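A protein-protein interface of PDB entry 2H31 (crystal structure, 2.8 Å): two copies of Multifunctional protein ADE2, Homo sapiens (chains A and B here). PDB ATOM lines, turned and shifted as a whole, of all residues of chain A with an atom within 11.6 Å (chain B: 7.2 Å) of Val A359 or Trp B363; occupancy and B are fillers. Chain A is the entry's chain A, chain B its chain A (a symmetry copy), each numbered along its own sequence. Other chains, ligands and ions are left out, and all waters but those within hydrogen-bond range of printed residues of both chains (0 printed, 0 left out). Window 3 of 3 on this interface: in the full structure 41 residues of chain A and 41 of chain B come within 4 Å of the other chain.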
ATOM      1  N   GLY A 330       2.207   8.487 -12.040  1.00  0.00           N
ATOM      2  CA  GLY A 330       2.496   9.289 -13.219  1.00  0.00           C
ATOM      3  C   GLY A 330       1.809   8.741 -14.462  1.00  0.00           C
ATOM      4  O   GLY A 330       1.299   7.609 -14.445  1.00  0.00           O
ATOM      5  N   ARG A 331       1.786   9.528 -15.539  1.00  0.00           N
ATOM      6  CA  ARG A 331       1.121   9.102 -16.772  1.00  0.00           C
ATOM      7  C   ARG A 331      -0.328   8.718 -16.464  1.00  0.00           C
ATOM      8  O   ARG A 331      -0.946   9.274 -15.553  1.00  0.00           O
ATOM      9  CB  ARG A 331       1.826   7.885 -17.384  1.00  0.00           C
ATOM     10  CG  ARG A 331       2.957   8.192 -18.333  1.00  0.00           C
ATOM     11  CD  ARG A 331       4.236   8.422 -17.596  1.00  0.00           C
ATOM     12  NE  ARG A 331       5.393   8.470 -18.491  1.00  0.00           N
ATOM     13  CZ  ARG A 331       5.618   7.606 -19.483  1.00  0.00           C
ATOM     14  NH1 ARG A 331       4.753   6.626 -19.731  1.00  0.00           N
ATOM     15  NH2 ARG A 331       6.736   7.694 -20.202  1.00  0.00           N
ATOM     16  N   SER A 332      -0.869   7.765 -17.220  1.00  0.00           N
ATOM     17  CA  SER A 332      -2.231   7.314 -16.973  1.00  0.00           C
ATOM     18  C   SER A 332      -2.310   6.716 -15.569  1.00  0.00           C
ATOM     19  O   SER A 332      -1.744   5.657 -15.278  1.00  0.00           O
ATOM     20  CB  SER A 332      -2.667   6.270 -17.992  1.00  0.00           C
ATOM     21  OG  SER A 332      -3.946   5.768 -17.643  1.00  0.00           O
ATOM     22  N   ASN A 333      -3.034   7.424 -14.716  1.00  0.00           N
ATOM     23  CA  ASN A 333      -3.222   7.068 -13.331  1.00  0.00           C
ATOM     24  C   ASN A 333      -4.397   6.120 -13.168  1.00  0.00           C
ATOM     25  O   ASN A 333      -5.557   6.524 -13.266  1.00  0.00           O
ATOM     26  CB  ASN A 333      -3.419   8.372 -12.547  1.00  0.00           C
ATOM     27  CG  ASN A 333      -3.970   8.170 -11.156  1.00  0.00           C
ATOM     28  OD1 ASN A 333      -4.157   7.046 -10.691  1.00  0.00           O
ATOM     29  ND2 ASN A 333      -4.235   9.278 -10.476  1.00  0.00           N
ATOM     30  N   PRO A 351      -1.253  13.457  -8.618  1.00  0.00           N
ATOM     31  CA  PRO A 351      -0.343  13.209  -9.734  1.00  0.00           C
ATOM     32  C   PRO A 351       0.894  14.067  -9.722  1.00  0.00           C
ATOM     33  O   PRO A 351       0.842  15.268  -9.436  1.00  0.00           O
ATOM     34  CB  PRO A 351      -1.195  13.507 -10.959  1.00  0.00           C
ATOM     35  CG  PRO A 351      -2.593  13.400 -10.461  1.00  0.00           C
ATOM     36  CD  PRO A 351      -2.508  14.033  -9.111  1.00  0.00           C
ATOM     37  N   PRO A 352       2.040  13.452 -10.020  1.00  0.00           N
ATOM     38  CA  PRO A 352       3.330  14.138 -10.066  1.00  0.00           C
ATOM     39  C   PRO A 352       3.496  14.697 -11.477  1.00  0.00           C
ATOM     40  O   PRO A 352       4.316  14.224 -12.255  1.00  0.00           O
ATOM     41  CB  PRO A 352       4.313  13.025  -9.759  1.00  0.00           C
ATOM     42  CG  PRO A 352       3.694  11.874 -10.440  1.00  0.00           C
ATOM     43  CD  PRO A 352       2.221  11.993 -10.071  1.00  0.00           C
ATOM     44  N   LEU A 353       2.690  15.701 -11.802  1.00  0.00           N
ATOM     45  CA  LEU A 353       2.717  16.331 -13.115  1.00  0.00           C
ATOM     46  C   LEU A 353       3.925  17.225 -13.312  1.00  0.00           C
ATOM     47  O   LEU A 353       4.457  17.777 -12.360  1.00  0.00           O
ATOM     48  CB  LEU A 353       1.483  17.204 -13.310  1.00  0.00           C
ATOM     49  CG  LEU A 353       0.109  16.667 -12.945  1.00  0.00           C
ATOM     50  CD1 LEU A 353      -0.837  17.839 -12.938  1.00  0.00           C
ATOM     51  CD2 LEU A 353      -0.345  15.578 -13.925  1.00  0.00           C
ATOM     52  N   THR A 354       4.348  17.366 -14.560  1.00  0.00           N
ATOM     53  CA  THR A 354       5.438  18.273 -14.903  1.00  0.00           C
ATOM     54  C   THR A 354       4.854  18.996 -16.116  1.00  0.00           C
ATOM     55  O   THR A 354       3.996  18.451 -16.813  1.00  0.00           O
ATOM     56  CB  THR A 354       6.733  17.526 -15.284  1.00  0.00           C
ATOM     57  OG1 THR A 354       6.653  17.051 -16.641  1.00  0.00           O
ATOM     58  CG2 THR A 354       6.947  16.370 -14.335  1.00  0.00           C
ATOM     59  N   PRO A 355       5.294  20.232 -16.384  1.00  0.00           N
ATOM     60  CA  PRO A 355       4.698  20.896 -17.553  1.00  0.00           C
ATOM     61  C   PRO A 355       4.935  20.234 -18.908  1.00  0.00           C
ATOM     62  O   PRO A 355       4.299  20.606 -19.893  1.00  0.00           O
ATOM     63  CB  PRO A 355       5.222  22.332 -17.456  1.00  0.00           C
ATOM     64  CG  PRO A 355       6.461  22.204 -16.662  1.00  0.00           C
ATOM     65  CD  PRO A 355       6.173  21.142 -15.636  1.00  0.00           C
ATOM     66  N   ASP A 356       5.821  19.239 -18.963  1.00  0.00           N
ATOM     67  CA  ASP A 356       6.052  18.540 -20.235  1.00  0.00           C
ATOM     68  C   ASP A 356       4.776  17.895 -20.795  1.00  0.00           C
ATOM     69  O   ASP A 356       4.338  18.236 -21.888  1.00  0.00           O
ATOM     70  CB  ASP A 356       7.129  17.468 -20.086  1.00  0.00           C
ATOM     71  CG  ASP A 356       8.510  18.016 -20.319  1.00  0.00           C
ATOM     72  OD1 ASP A 356       8.628  19.042 -21.022  1.00  0.00           O
ATOM     73  OD2 ASP A 356       9.480  17.415 -19.817  1.00  0.00           O
ATOM     74  N   TRP A 357       4.191  16.958 -20.050  1.00  0.00           N
ATOM     75  CA  TRP A 357       2.963  16.305 -20.498  1.00  0.00           C
ATOM     76  C   TRP A 357       1.843  16.389 -19.477  1.00  0.00           C
ATOM     77  O   TRP A 357       0.839  15.678 -19.597  1.00  0.00           O
ATOM     78  CB  TRP A 357       3.205  14.841 -20.800  1.00  0.00           C
ATOM     79  CG  TRP A 357       4.160  14.595 -21.882  1.00  0.00           C
ATOM     80  CD1 TRP A 357       5.510  14.428 -21.767  1.00  0.00           C
ATOM     81  CD2 TRP A 357       3.845  14.432 -23.254  1.00  0.00           C
ATOM     82  NE1 TRP A 357       6.056  14.163 -22.992  1.00  0.00           N
ATOM     83  CE2 TRP A 357       5.056  14.157 -23.927  1.00  0.00           C
ATOM     84  CE3 TRP A 357       2.651  14.485 -23.986  1.00  0.00           C
ATOM     85  CZ2 TRP A 357       5.114  13.931 -25.306  1.00  0.00           C
ATOM     86  CZ3 TRP A 357       2.700  14.258 -25.364  1.00  0.00           C
ATOM     87  CH2 TRP A 357       3.931  13.983 -26.009  1.00  0.00           C
ATOM     88  N   GLY A 358       2.027  17.262 -18.487  1.00  0.00           N
ATOM     89  CA  GLY A 358       1.058  17.433 -17.422  1.00  0.00           C
ATOM     90  C   GLY A 358      -0.362  17.612 -17.899  1.00  0.00           C
ATOM     91  O   GLY A 358      -1.273  16.926 -17.428  1.00  0.00           O
ATOM     92  N   VAL A 359      -0.552  18.544 -18.828  1.00  0.00           N
ATOM     93  CA  VAL A 359      -1.866  18.819 -19.382  1.00  0.00           C
ATOM     94  C   VAL A 359      -2.524  17.578 -19.969  1.00  0.00           C
ATOM     95  O   VAL A 359      -3.748  17.478 -20.022  1.00  0.00           O
ATOM     96  CB  VAL A 359      -1.772  19.919 -20.441  1.00  0.00           C
ATOM     97  CG1 VAL A 359      -2.947  19.858 -21.401  1.00  0.00           C
ATOM     98  CG2 VAL A 359      -1.737  21.257 -19.735  1.00  0.00           C
ATOM     99  N   GLN A 360      -1.727  16.618 -20.407  1.00  0.00           N
ATOM    100  CA  GLN A 360      -2.330  15.410 -20.941  1.00  0.00           C
ATOM    101  C   GLN A 360      -2.631  14.380 -19.843  1.00  0.00           C
ATOM    102  O   GLN A 360      -3.655  13.689 -19.891  1.00  0.00           O
ATOM    103  CB  GLN A 360      -1.433  14.790 -22.009  1.00  0.00           C
ATOM    104  CG  GLN A 360      -1.409  15.545 -23.331  1.00  0.00           C
ATOM    105  CD  GLN A 360      -0.862  16.969 -23.229  1.00  0.00           C
ATOM    106  OE1 GLN A 360       0.157  17.230 -22.568  1.00  0.00           O
ATOM    107  NE2 GLN A 360      -1.531  17.895 -23.910  1.00  0.00           N
ATOM    108  N   ASP A 361      -1.757  14.301 -18.844  1.00  0.00           N
ATOM    109  CA  ASP A 361      -1.942  13.331 -17.782  1.00  0.00           C
ATOM    110  C   ASP A 361      -3.021  13.590 -16.735  1.00  0.00           C
ATOM    111  O   ASP A 361      -3.693  12.640 -16.337  1.00  0.00           O
ATOM    112  CB  ASP A 361      -0.612  13.057 -17.080  1.00  0.00           C
ATOM    113  CG  ASP A 361       0.452  12.508 -18.029  1.00  0.00           C
ATOM    114  OD1 ASP A 361       0.079  11.819 -19.013  1.00  0.00           O
ATOM    115  OD2 ASP A 361       1.664  12.748 -17.784  1.00  0.00           O
ATOM    116  N   VAL A 362      -3.221  14.832 -16.290  1.00  0.00           N
ATOM    117  CA  VAL A 362      -4.236  15.070 -15.253  1.00  0.00           C
ATOM    118  C   VAL A 362      -5.586  14.446 -15.531  1.00  0.00           C
ATOM    119  O   VAL A 362      -6.262  13.990 -14.608  1.00  0.00           O
ATOM    120  CB  VAL A 362      -4.572  16.564 -15.000  1.00  0.00           C
ATOM    121  CG1 VAL A 362      -3.459  17.236 -14.272  1.00  0.00           C
ATOM    122  CG2 VAL A 362      -4.927  17.266 -16.320  1.00  0.00           C
ATOM    123  N   TRP A 363      -6.001  14.460 -16.794  1.00  0.00           N
ATOM    124  CA  TRP A 363      -7.310  13.927 -17.123  1.00  0.00           C
ATOM    125  C   TRP A 363      -7.539  12.459 -16.774  1.00  0.00           C
ATOM    126  O   TRP A 363      -8.693  12.019 -16.664  1.00  0.00           O
ATOM    127  CB  TRP A 363      -7.637  14.196 -18.586  1.00  0.00           C
ATOM    128  CG  TRP A 363      -7.819  15.635 -18.865  1.00  0.00           C
ATOM    129  CD1 TRP A 363      -6.899  16.491 -19.391  1.00  0.00           C
ATOM    130  CD2 TRP A 363      -8.985  16.413 -18.594  1.00  0.00           C
ATOM    131  NE1 TRP A 363      -7.420  17.760 -19.467  1.00  0.00           N
ATOM    132  CE2 TRP A 363      -8.700  17.743 -18.983  1.00  0.00           C
ATOM    133  CE3 TRP A 363     -10.247  16.120 -18.056  1.00  0.00           C
ATOM    134  CZ2 TRP A 363      -9.630  18.778 -18.851  1.00  0.00           C
ATOM    135  CZ3 TRP A 363     -11.172  17.147 -17.922  1.00  0.00           C
ATOM    136  CH2 TRP A 363     -10.859  18.462 -18.319  1.00  0.00           C
ATOM    137  N   SER A 364      -6.470  11.695 -16.587  1.00  0.00           N
ATOM    138  CA  SER A 364      -6.685  10.308 -16.229  1.00  0.00           C
ATOM    139  C   SER A 364      -7.089  10.247 -14.771  1.00  0.00           C
ATOM    140  O   SER A 364      -7.650   9.253 -14.335  1.00  0.00           O
ATOM    141  CB  SER A 364      -5.438   9.461 -16.464  1.00  0.00           C
ATOM    142  OG  SER A 364      -4.426   9.784 -15.535  1.00  0.00           O
ATOM    143  N   SER A 365      -6.806  11.309 -14.019  1.00  0.00           N
ATOM    144  CA  SER A 365      -7.161  11.384 -12.598  1.00  0.00           C
ATOM    145  C   SER A 365      -8.510  12.047 -12.427  1.00  0.00           C
ATOM    146  O   SER A 365      -9.205  11.786 -11.470  1.00  0.00           O
ATOM    147  CB  SER A 365      -6.108  12.149 -11.806  1.00  0.00           C
ATOM    148  OG  SER A 365      -4.861  11.481 -11.875  1.00  0.00           O
ATOM    149  N   LEU A 366      -8.858  12.939 -13.342  1.00  0.00           N
ATOM    150  CA  LEU A 366     -10.163  13.588 -13.349  1.00  0.00           C
ATOM    151  C   LEU A 366     -10.855  12.627 -14.305  1.00  0.00           C
ATOM    152  O   LEU A 366     -10.228  11.647 -14.715  1.00  0.00           O
ATOM    153  CB  LEU A 366     -10.069  14.942 -14.024  1.00  0.00           C
ATOM    154  CG  LEU A 366      -8.881  15.857 -13.722  1.00  0.00           C
ATOM    155  CD1 LEU A 366      -8.850  16.961 -14.779  1.00  0.00           C
ATOM    156  CD2 LEU A 366      -8.989  16.443 -12.301  1.00  0.00           C
ATOM    157  N   ARG A 367     -12.106  12.864 -14.686  1.00  0.00           N
ATOM    158  CA  ARG A 367     -12.781  11.965 -15.651  1.00  0.00           C
ATOM    159  C   ARG A 367     -12.679  10.465 -15.317  1.00  0.00           C
ATOM    160  O   ARG A 367     -11.978   9.717 -15.988  1.00  0.00           O
ATOM    161  CB  ARG A 367     -12.202  12.181 -17.045  1.00  0.00           C
ATOM    162  CG  ARG A 367     -12.228  13.609 -17.537  1.00  0.00           C
ATOM    163  CD  ARG A 367     -13.515  13.923 -18.260  1.00  0.00           C
ATOM    164  NE  ARG A 367     -13.781  12.922 -19.283  1.00  0.00           N
ATOM    165  CZ  ARG A 367     -14.933  12.817 -19.929  1.00  0.00           C
ATOM    166  NH1 ARG A 367     -15.921  13.657 -19.662  1.00  0.00           N
ATOM    167  NH2 ARG A 367     -15.105  11.860 -20.826  1.00  0.00           N
ATOM    168  N   THR A 376      -9.135  14.787  -6.742  1.00  0.00           N
ATOM    169  CA  THR A 376      -7.811  15.144  -7.217  1.00  0.00           C
ATOM    170  C   THR A 376      -7.283  16.409  -6.538  1.00  0.00           C
ATOM    171  O   THR A 376      -8.050  17.328  -6.266  1.00  0.00           O
ATOM    172  CB  THR A 376      -7.836  15.373  -8.733  1.00  0.00           C
ATOM    173  OG1 THR A 376      -8.418  14.234  -9.382  1.00  0.00           O
ATOM    174  CG2 THR A 376      -6.426  15.594  -9.257  1.00  0.00           C
ATOM    175  N   VAL A 377      -5.986  16.426  -6.238  1.00  0.00           N
ATOM    176  CA  VAL A 377      -5.312  17.592  -5.647  1.00  0.00           C
ATOM    177  C   VAL A 377      -3.900  17.601  -6.200  1.00  0.00           C
ATOM    178  O   VAL A 377      -3.102  16.706  -5.902  1.00  0.00           O
ATOM    179  CB  VAL A 377      -5.211  17.551  -4.110  1.00  0.00           C
ATOM    180  CG1 VAL A 377      -4.333  18.671  -3.640  1.00  0.00           C
ATOM    181  CG2 VAL A 377      -6.570  17.727  -3.480  1.00  0.00           C
ATOM    182  N   LEU A 378      -3.580  18.611  -7.005  1.00  0.00           N
ATOM    183  CA  LEU A 378      -2.262  18.666  -7.621  1.00  0.00           C
ATOM    184  C   LEU A 378      -1.075  18.914  -6.686  1.00  0.00           C
ATOM    185  O   LEU A 378      -0.048  18.238  -6.808  1.00  0.00           O
ATOM    186  CB  LEU A 378      -2.269  19.695  -8.750  1.00  0.00           C
ATOM    187  CG  LEU A 378      -3.348  19.397  -9.793  1.00  0.00           C
ATOM    188  CD1 LEU A 378      -3.371  20.463 -10.850  1.00  0.00           C
ATOM    189  CD2 LEU A 378      -3.082  18.052 -10.410  1.00  0.00           C
ATOM    190  N   SER A 379      -1.212  19.860  -5.752  1.00  0.00           N
ATOM    191  CA  SER A 379      -0.124  20.193  -4.832  1.00  0.00           C
ATOM    192  C   SER A 379       0.170  19.086  -3.834  1.00  0.00           C
ATOM    193  O   SER A 379      -0.722  18.641  -3.109  1.00  0.00           O
ATOM    194  CB  SER A 379      -0.447  21.479  -4.071  1.00  0.00           C
ATOM    195  OG  SER A 379       0.634  21.862  -3.235  1.00  0.00           O
ATOM    196  N   ASN B 333     -13.593  29.699 -11.158  1.00  0.00           N
ATOM    197  CA  ASN B 333     -14.038  29.324  -9.838  1.00  0.00           C
ATOM    198  C   ASN B 333     -13.150  29.939  -8.769  1.00  0.00           C
ATOM    199  O   ASN B 333     -12.016  29.505  -8.559  1.00  0.00           O
ATOM    200  CB  ASN B 333     -14.038  27.791  -9.775  1.00  0.00           C
ATOM    201  CG  ASN B 333     -14.139  27.238  -8.374  1.00  0.00           C
ATOM    202  OD1 ASN B 333     -14.289  27.972  -7.398  1.00  0.00           O
ATOM    203  ND2 ASN B 333     -14.057  25.918  -8.270  1.00  0.00           N
ATOM    204  N   LEU B 353     -19.043  21.740 -15.245  1.00  0.00           N
ATOM    205  CA  LEU B 353     -18.453  21.825 -16.575  1.00  0.00           C
ATOM    206  C   LEU B 353     -19.362  21.277 -17.657  1.00  0.00           C
ATOM    207  O   LEU B 353     -20.175  20.400 -17.405  1.00  0.00           O
ATOM    208  CB  LEU B 353     -17.160  21.021 -16.632  1.00  0.00           C
ATOM    209  CG  LEU B 353     -16.130  21.159 -15.524  1.00  0.00           C
ATOM    210  CD1 LEU B 353     -15.147  20.030 -15.688  1.00  0.00           C
ATOM    211  CD2 LEU B 353     -15.436  22.526 -15.571  1.00  0.00           C
ATOM    212  N   GLY B 358     -15.500  23.514 -20.890  1.00  0.00           N
ATOM    213  CA  GLY B 358     -15.047  22.746 -19.746  1.00  0.00           C
ATOM    214  C   GLY B 358     -13.546  22.660 -19.614  1.00  0.00           C
ATOM    215  O   GLY B 358     -12.995  22.929 -18.543  1.00  0.00           O
ATOM    216  N   VAL B 359     -12.886  22.274 -20.700  1.00  0.00           N
ATOM    217  CA  VAL B 359     -11.438  22.153 -20.717  1.00  0.00           C
ATOM    218  C   VAL B 359     -10.740  23.441 -20.302  1.00  0.00           C
ATOM    219  O   VAL B 359      -9.624  23.416 -19.788  1.00  0.00           O
ATOM    220  CB  VAL B 359     -10.961  21.714 -22.102  1.00  0.00           C
ATOM    221  CG1 VAL B 359      -9.510  22.096 -22.329  1.00  0.00           C
ATOM    222  CG2 VAL B 359     -11.135  20.214 -22.212  1.00  0.00           C
ATOM    223  N   GLN B 360     -11.386  24.575 -20.511  1.00  0.00           N
ATOM    224  CA  GLN B 360     -10.755  25.815 -20.095  1.00  0.00           C
ATOM    225  C   GLN B 360     -11.054  26.151 -18.626  1.00  0.00           C
ATOM    226  O   GLN B 360     -10.186  26.661 -17.908  1.00  0.00           O
ATOM    227  CB  GLN B 360     -11.193  26.968 -20.995  1.00  0.00           C
ATOM    228  CG  GLN B 360     -10.582  26.948 -22.389  1.00  0.00           C
ATOM    229  CD  GLN B 360     -10.958  25.720 -23.221  1.00  0.00           C
ATOM    230  OE1 GLN B 360     -12.123  25.290 -23.257  1.00  0.00           O
ATOM    231  NE2 GLN B 360      -9.968  25.166 -23.914  1.00  0.00           N
ATOM    232  N   ASP B 361     -12.266  25.838 -18.179  1.00  0.00           N
ATOM    233  CA  ASP B 361     -12.648  26.152 -16.815  1.00  0.00           C
ATOM    234  C   ASP B 361     -12.078  25.305 -15.682  1.00  0.00           C
ATOM    235  O   ASP B 361     -11.742  25.865 -14.640  1.00  0.00           O
ATOM    236  CB  ASP B 361     -14.170  26.203 -16.692  1.00  0.00           C
ATOM    237  CG  ASP B 361     -14.799  27.256 -17.603  1.00  0.00           C
ATOM    238  OD1 ASP B 361     -14.132  28.285 -17.879  1.00  0.00           O
ATOM    239  OD2 ASP B 361     -15.969  27.065 -18.031  1.00  0.00           O
ATOM    240  N   VAL B 362     -11.942  23.987 -15.851  1.00  0.00           N
ATOM    241  CA  VAL B 362     -11.429  23.169 -14.742  1.00  0.00           C
ATOM    242  C   VAL B 362     -10.164  23.694 -14.099  1.00  0.00           C
ATOM    243  O   VAL B 362      -9.987  23.573 -12.886  1.00  0.00           O
ATOM    244  CB  VAL B 362     -11.063  21.710 -15.124  1.00  0.00           C
ATOM    245  CG1 VAL B 362     -12.294  20.900 -15.344  1.00  0.00           C
ATOM    246  CG2 VAL B 362     -10.116  21.692 -16.335  1.00  0.00           C
ATOM    247  N   TRP B 363      -9.264  24.242 -14.911  1.00  0.00           N
ATOM    248  CA  TRP B 363      -8.006  24.716 -14.367  1.00  0.00           C
ATOM    249  C   TRP B 363      -8.107  25.801 -13.298  1.00  0.00           C
ATOM    250  O   TRP B 363      -7.161  26.001 -12.523  1.00  0.00           O
ATOM    251  CB  TRP B 363      -7.073  25.147 -15.492  1.00  0.00           C
ATOM    252  CG  TRP B 363      -6.633  24.009 -16.323  1.00  0.00           C
ATOM    253  CD1 TRP B 363      -7.150  23.619 -17.521  1.00  0.00           C
ATOM    254  CD2 TRP B 363      -5.604  23.070 -16.004  1.00  0.00           C
ATOM    255  NE1 TRP B 363      -6.505  22.493 -17.973  1.00  0.00           N
ATOM    256  CE2 TRP B 363      -5.552  22.132 -17.061  1.00  0.00           C
ATOM    257  CE3 TRP B 363      -4.720  22.927 -14.924  1.00  0.00           C
ATOM    258  CZ2 TRP B 363      -4.650  21.064 -17.070  1.00  0.00           C
ATOM    259  CZ3 TRP B 363      -3.825  21.865 -14.930  1.00  0.00           C
ATOM    260  CH2 TRP B 363      -3.796  20.945 -15.997  1.00  0.00           C
ATOM    261  N   SER B 364      -9.236  26.496 -13.230  1.00  0.00           N
ATOM    262  CA  SER B 364      -9.346  27.507 -12.198  1.00  0.00           C
ATOM    263  C   SER B 364      -9.592  26.815 -10.874  1.00  0.00           C
ATOM    264  O   SER B 364      -9.377  27.408  -9.828  1.00  0.00           O
ATOM    265  CB  SER B 364     -10.470  28.496 -12.490  1.00  0.00           C
ATOM    266  OG  SER B 364     -11.733  27.883 -12.347  1.00  0.00           O
ATOM    267  N   SER B 365     -10.040  25.562 -10.919  1.00  0.00           N
ATOM    268  CA  SER B 365     -10.300  24.776  -9.709  1.00  0.00           C
ATOM    269  C   SER B 365      -9.078  23.965  -9.336  1.00  0.00           C
ATOM    270  O   SER B 365      -8.876  23.655  -8.182  1.00  0.00           O
ATOM    271  CB  SER B 365     -11.493  23.847  -9.900  1.00  0.00           C
ATOM    272  OG  SER B 365     -12.665  24.602 -10.150  1.00  0.00           O
ATOM    273  N   LEU B 366      -8.284  23.589 -10.327  1.00  0.00           N
ATOM    274  CA  LEU B 366      -7.030  22.881 -10.103  1.00  0.00           C
ATOM    275  C   LEU B 366      -6.116  24.099 -10.095  1.00  0.00           C
ATOM    276  O   LEU B 366      -6.623  25.218 -10.202  1.00  0.00           O
ATOM    277  CB  LEU B 366      -6.683  22.037 -11.314  1.00  0.00           C
ATOM    278  CG  LEU B 366      -7.780  21.229 -12.011  1.00  0.00           C
ATOM    279  CD1 LEU B 366      -7.246  20.779 -13.371  1.00  0.00           C
ATOM    280  CD2 LEU B 366      -8.204  20.025 -11.148  1.00  0.00           C
ATOM    281  N   ARG B 367      -4.802  23.935  -9.985  1.00  0.00           N
ATOM    282  CA  ARG B 367      -3.894  25.104 -10.021  1.00  0.00           C
ATOM    283  C   ARG B 367      -4.292  26.261  -9.085  1.00  0.00           C
ATOM    284  O   ARG B 367      -4.731  27.313  -9.535  1.00  0.00           O
ATOM    285  CB  ARG B 367      -3.815  25.650 -11.443  1.00  0.00           C
ATOM    286  CG  ARG B 367      -3.428  24.640 -12.497  1.00  0.00           C
ATOM    287  CD  ARG B 367      -1.930  24.570 -12.674  1.00  0.00           C
ATOM    288  NE  ARG B 367      -1.378  25.902 -12.875  1.00  0.00           N
ATOM    289  CZ  ARG B 367      -0.082  26.174 -12.847  1.00  0.00           C
ATOM    290  NH1 ARG B 367       0.794  25.204 -12.633  1.00  0.00           N
ATOM    291  NH2 ARG B 367       0.337  27.418 -13.010  1.00  0.00           N
ATOM    292  N   LEU B 368      -4.129  26.062  -7.784  1.00  0.00           N
ATOM    293  CA  LEU B 368      -4.471  27.079  -6.798  1.00  0.00           C
ATOM    294  C   LEU B 368      -3.187  27.563  -6.158  1.00  0.00           C
ATOM    295  O   LEU B 368      -2.188  26.854  -6.141  1.00  0.00           O
ATOM    296  CB  LEU B 368      -5.367  26.486  -5.710  1.00  0.00           C
ATOM    297  CG  LEU B 368      -6.734  25.929  -6.111  1.00  0.00           C
ATOM    298  CD1 LEU B 368      -6.557  24.843  -7.123  1.00  0.00           C
ATOM    299  CD2 LEU B 368      -7.448  25.372  -4.897  1.00  0.00           C
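Among the printed residues, pairs that only touch across the chains: Val A359 with Trp B363 (3.95 Å), Val A362 with Trp B363 (3.9 Å), Trp A363 with Val B359 (3.95 Å), Trp A363 with Val B362 (3.9 Å), Leu A366 with Leu B366 (3.8 Å), Leu A378 with Leu B366 (3.7 Å) and Leu A378 with Arg B367 (3.9 Å).
Asp A356 touches none of the printed residues of chain B.
No residue of chain B comes within 4 Å of Gly A358.
Val A359 touches one residue of chain B.
Printed residues of chain B within 4 Å of Val A362: Trp B363.
Printed residues of chain B within 4 Å of Leu A366: Leu B366.
Trp B363 touches just these residues of chain A: Val A359 (3.95 Å) and Val A362 (3.9 Å).
Ser B364 touches none of the printed residues of chain A.
No residue of chain A comes within 4 Å of Ser B365.
Arg B367 touches just one residue of chain A: Leu A378.
Of the 25 printed residues of chain A, 5 touch a printed residue of chain B.
Printed residues of chain A that touch a printed residue of chain B: Val A359, Val A362, Trp A363, Leu A366 and Leu A378.
Hydrophobic or aromatic side chains of chain A that line the printed part of chain B: Val A359, Val A362, Trp A363, Leu A366 and Leu A378.
Of the 13 printed residues of chain B, 5 touch a printed residue of chain A.
Printed residues of chain B that touch a printed residue of chain A: Val B359, Val B362, Trp B363, Leu B366 and Arg B367.
Hydrophobic or aromatic side chains of chain B within 4 Å of the printed part of chain A: Val B359, Val B362, Trp B363 and Leu B366.
Among the printed residues, no Asp or Glu carboxylate lies within 4 Å of a Lys or Arg side-chain nitrogen of the other chain.
Val A359 touches Trp B363, and with the chains exchanged Trp A363 touches Val B359.
Val A362 touches Trp B363, and with the chains exchanged Trp A363 touches Val B362.
Leu A366 touches its own counterpart, Leu B366.
Of the 7 pairs that touch across the chains among the printed residues, 5 have their exchanged pair printed and touching as well.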
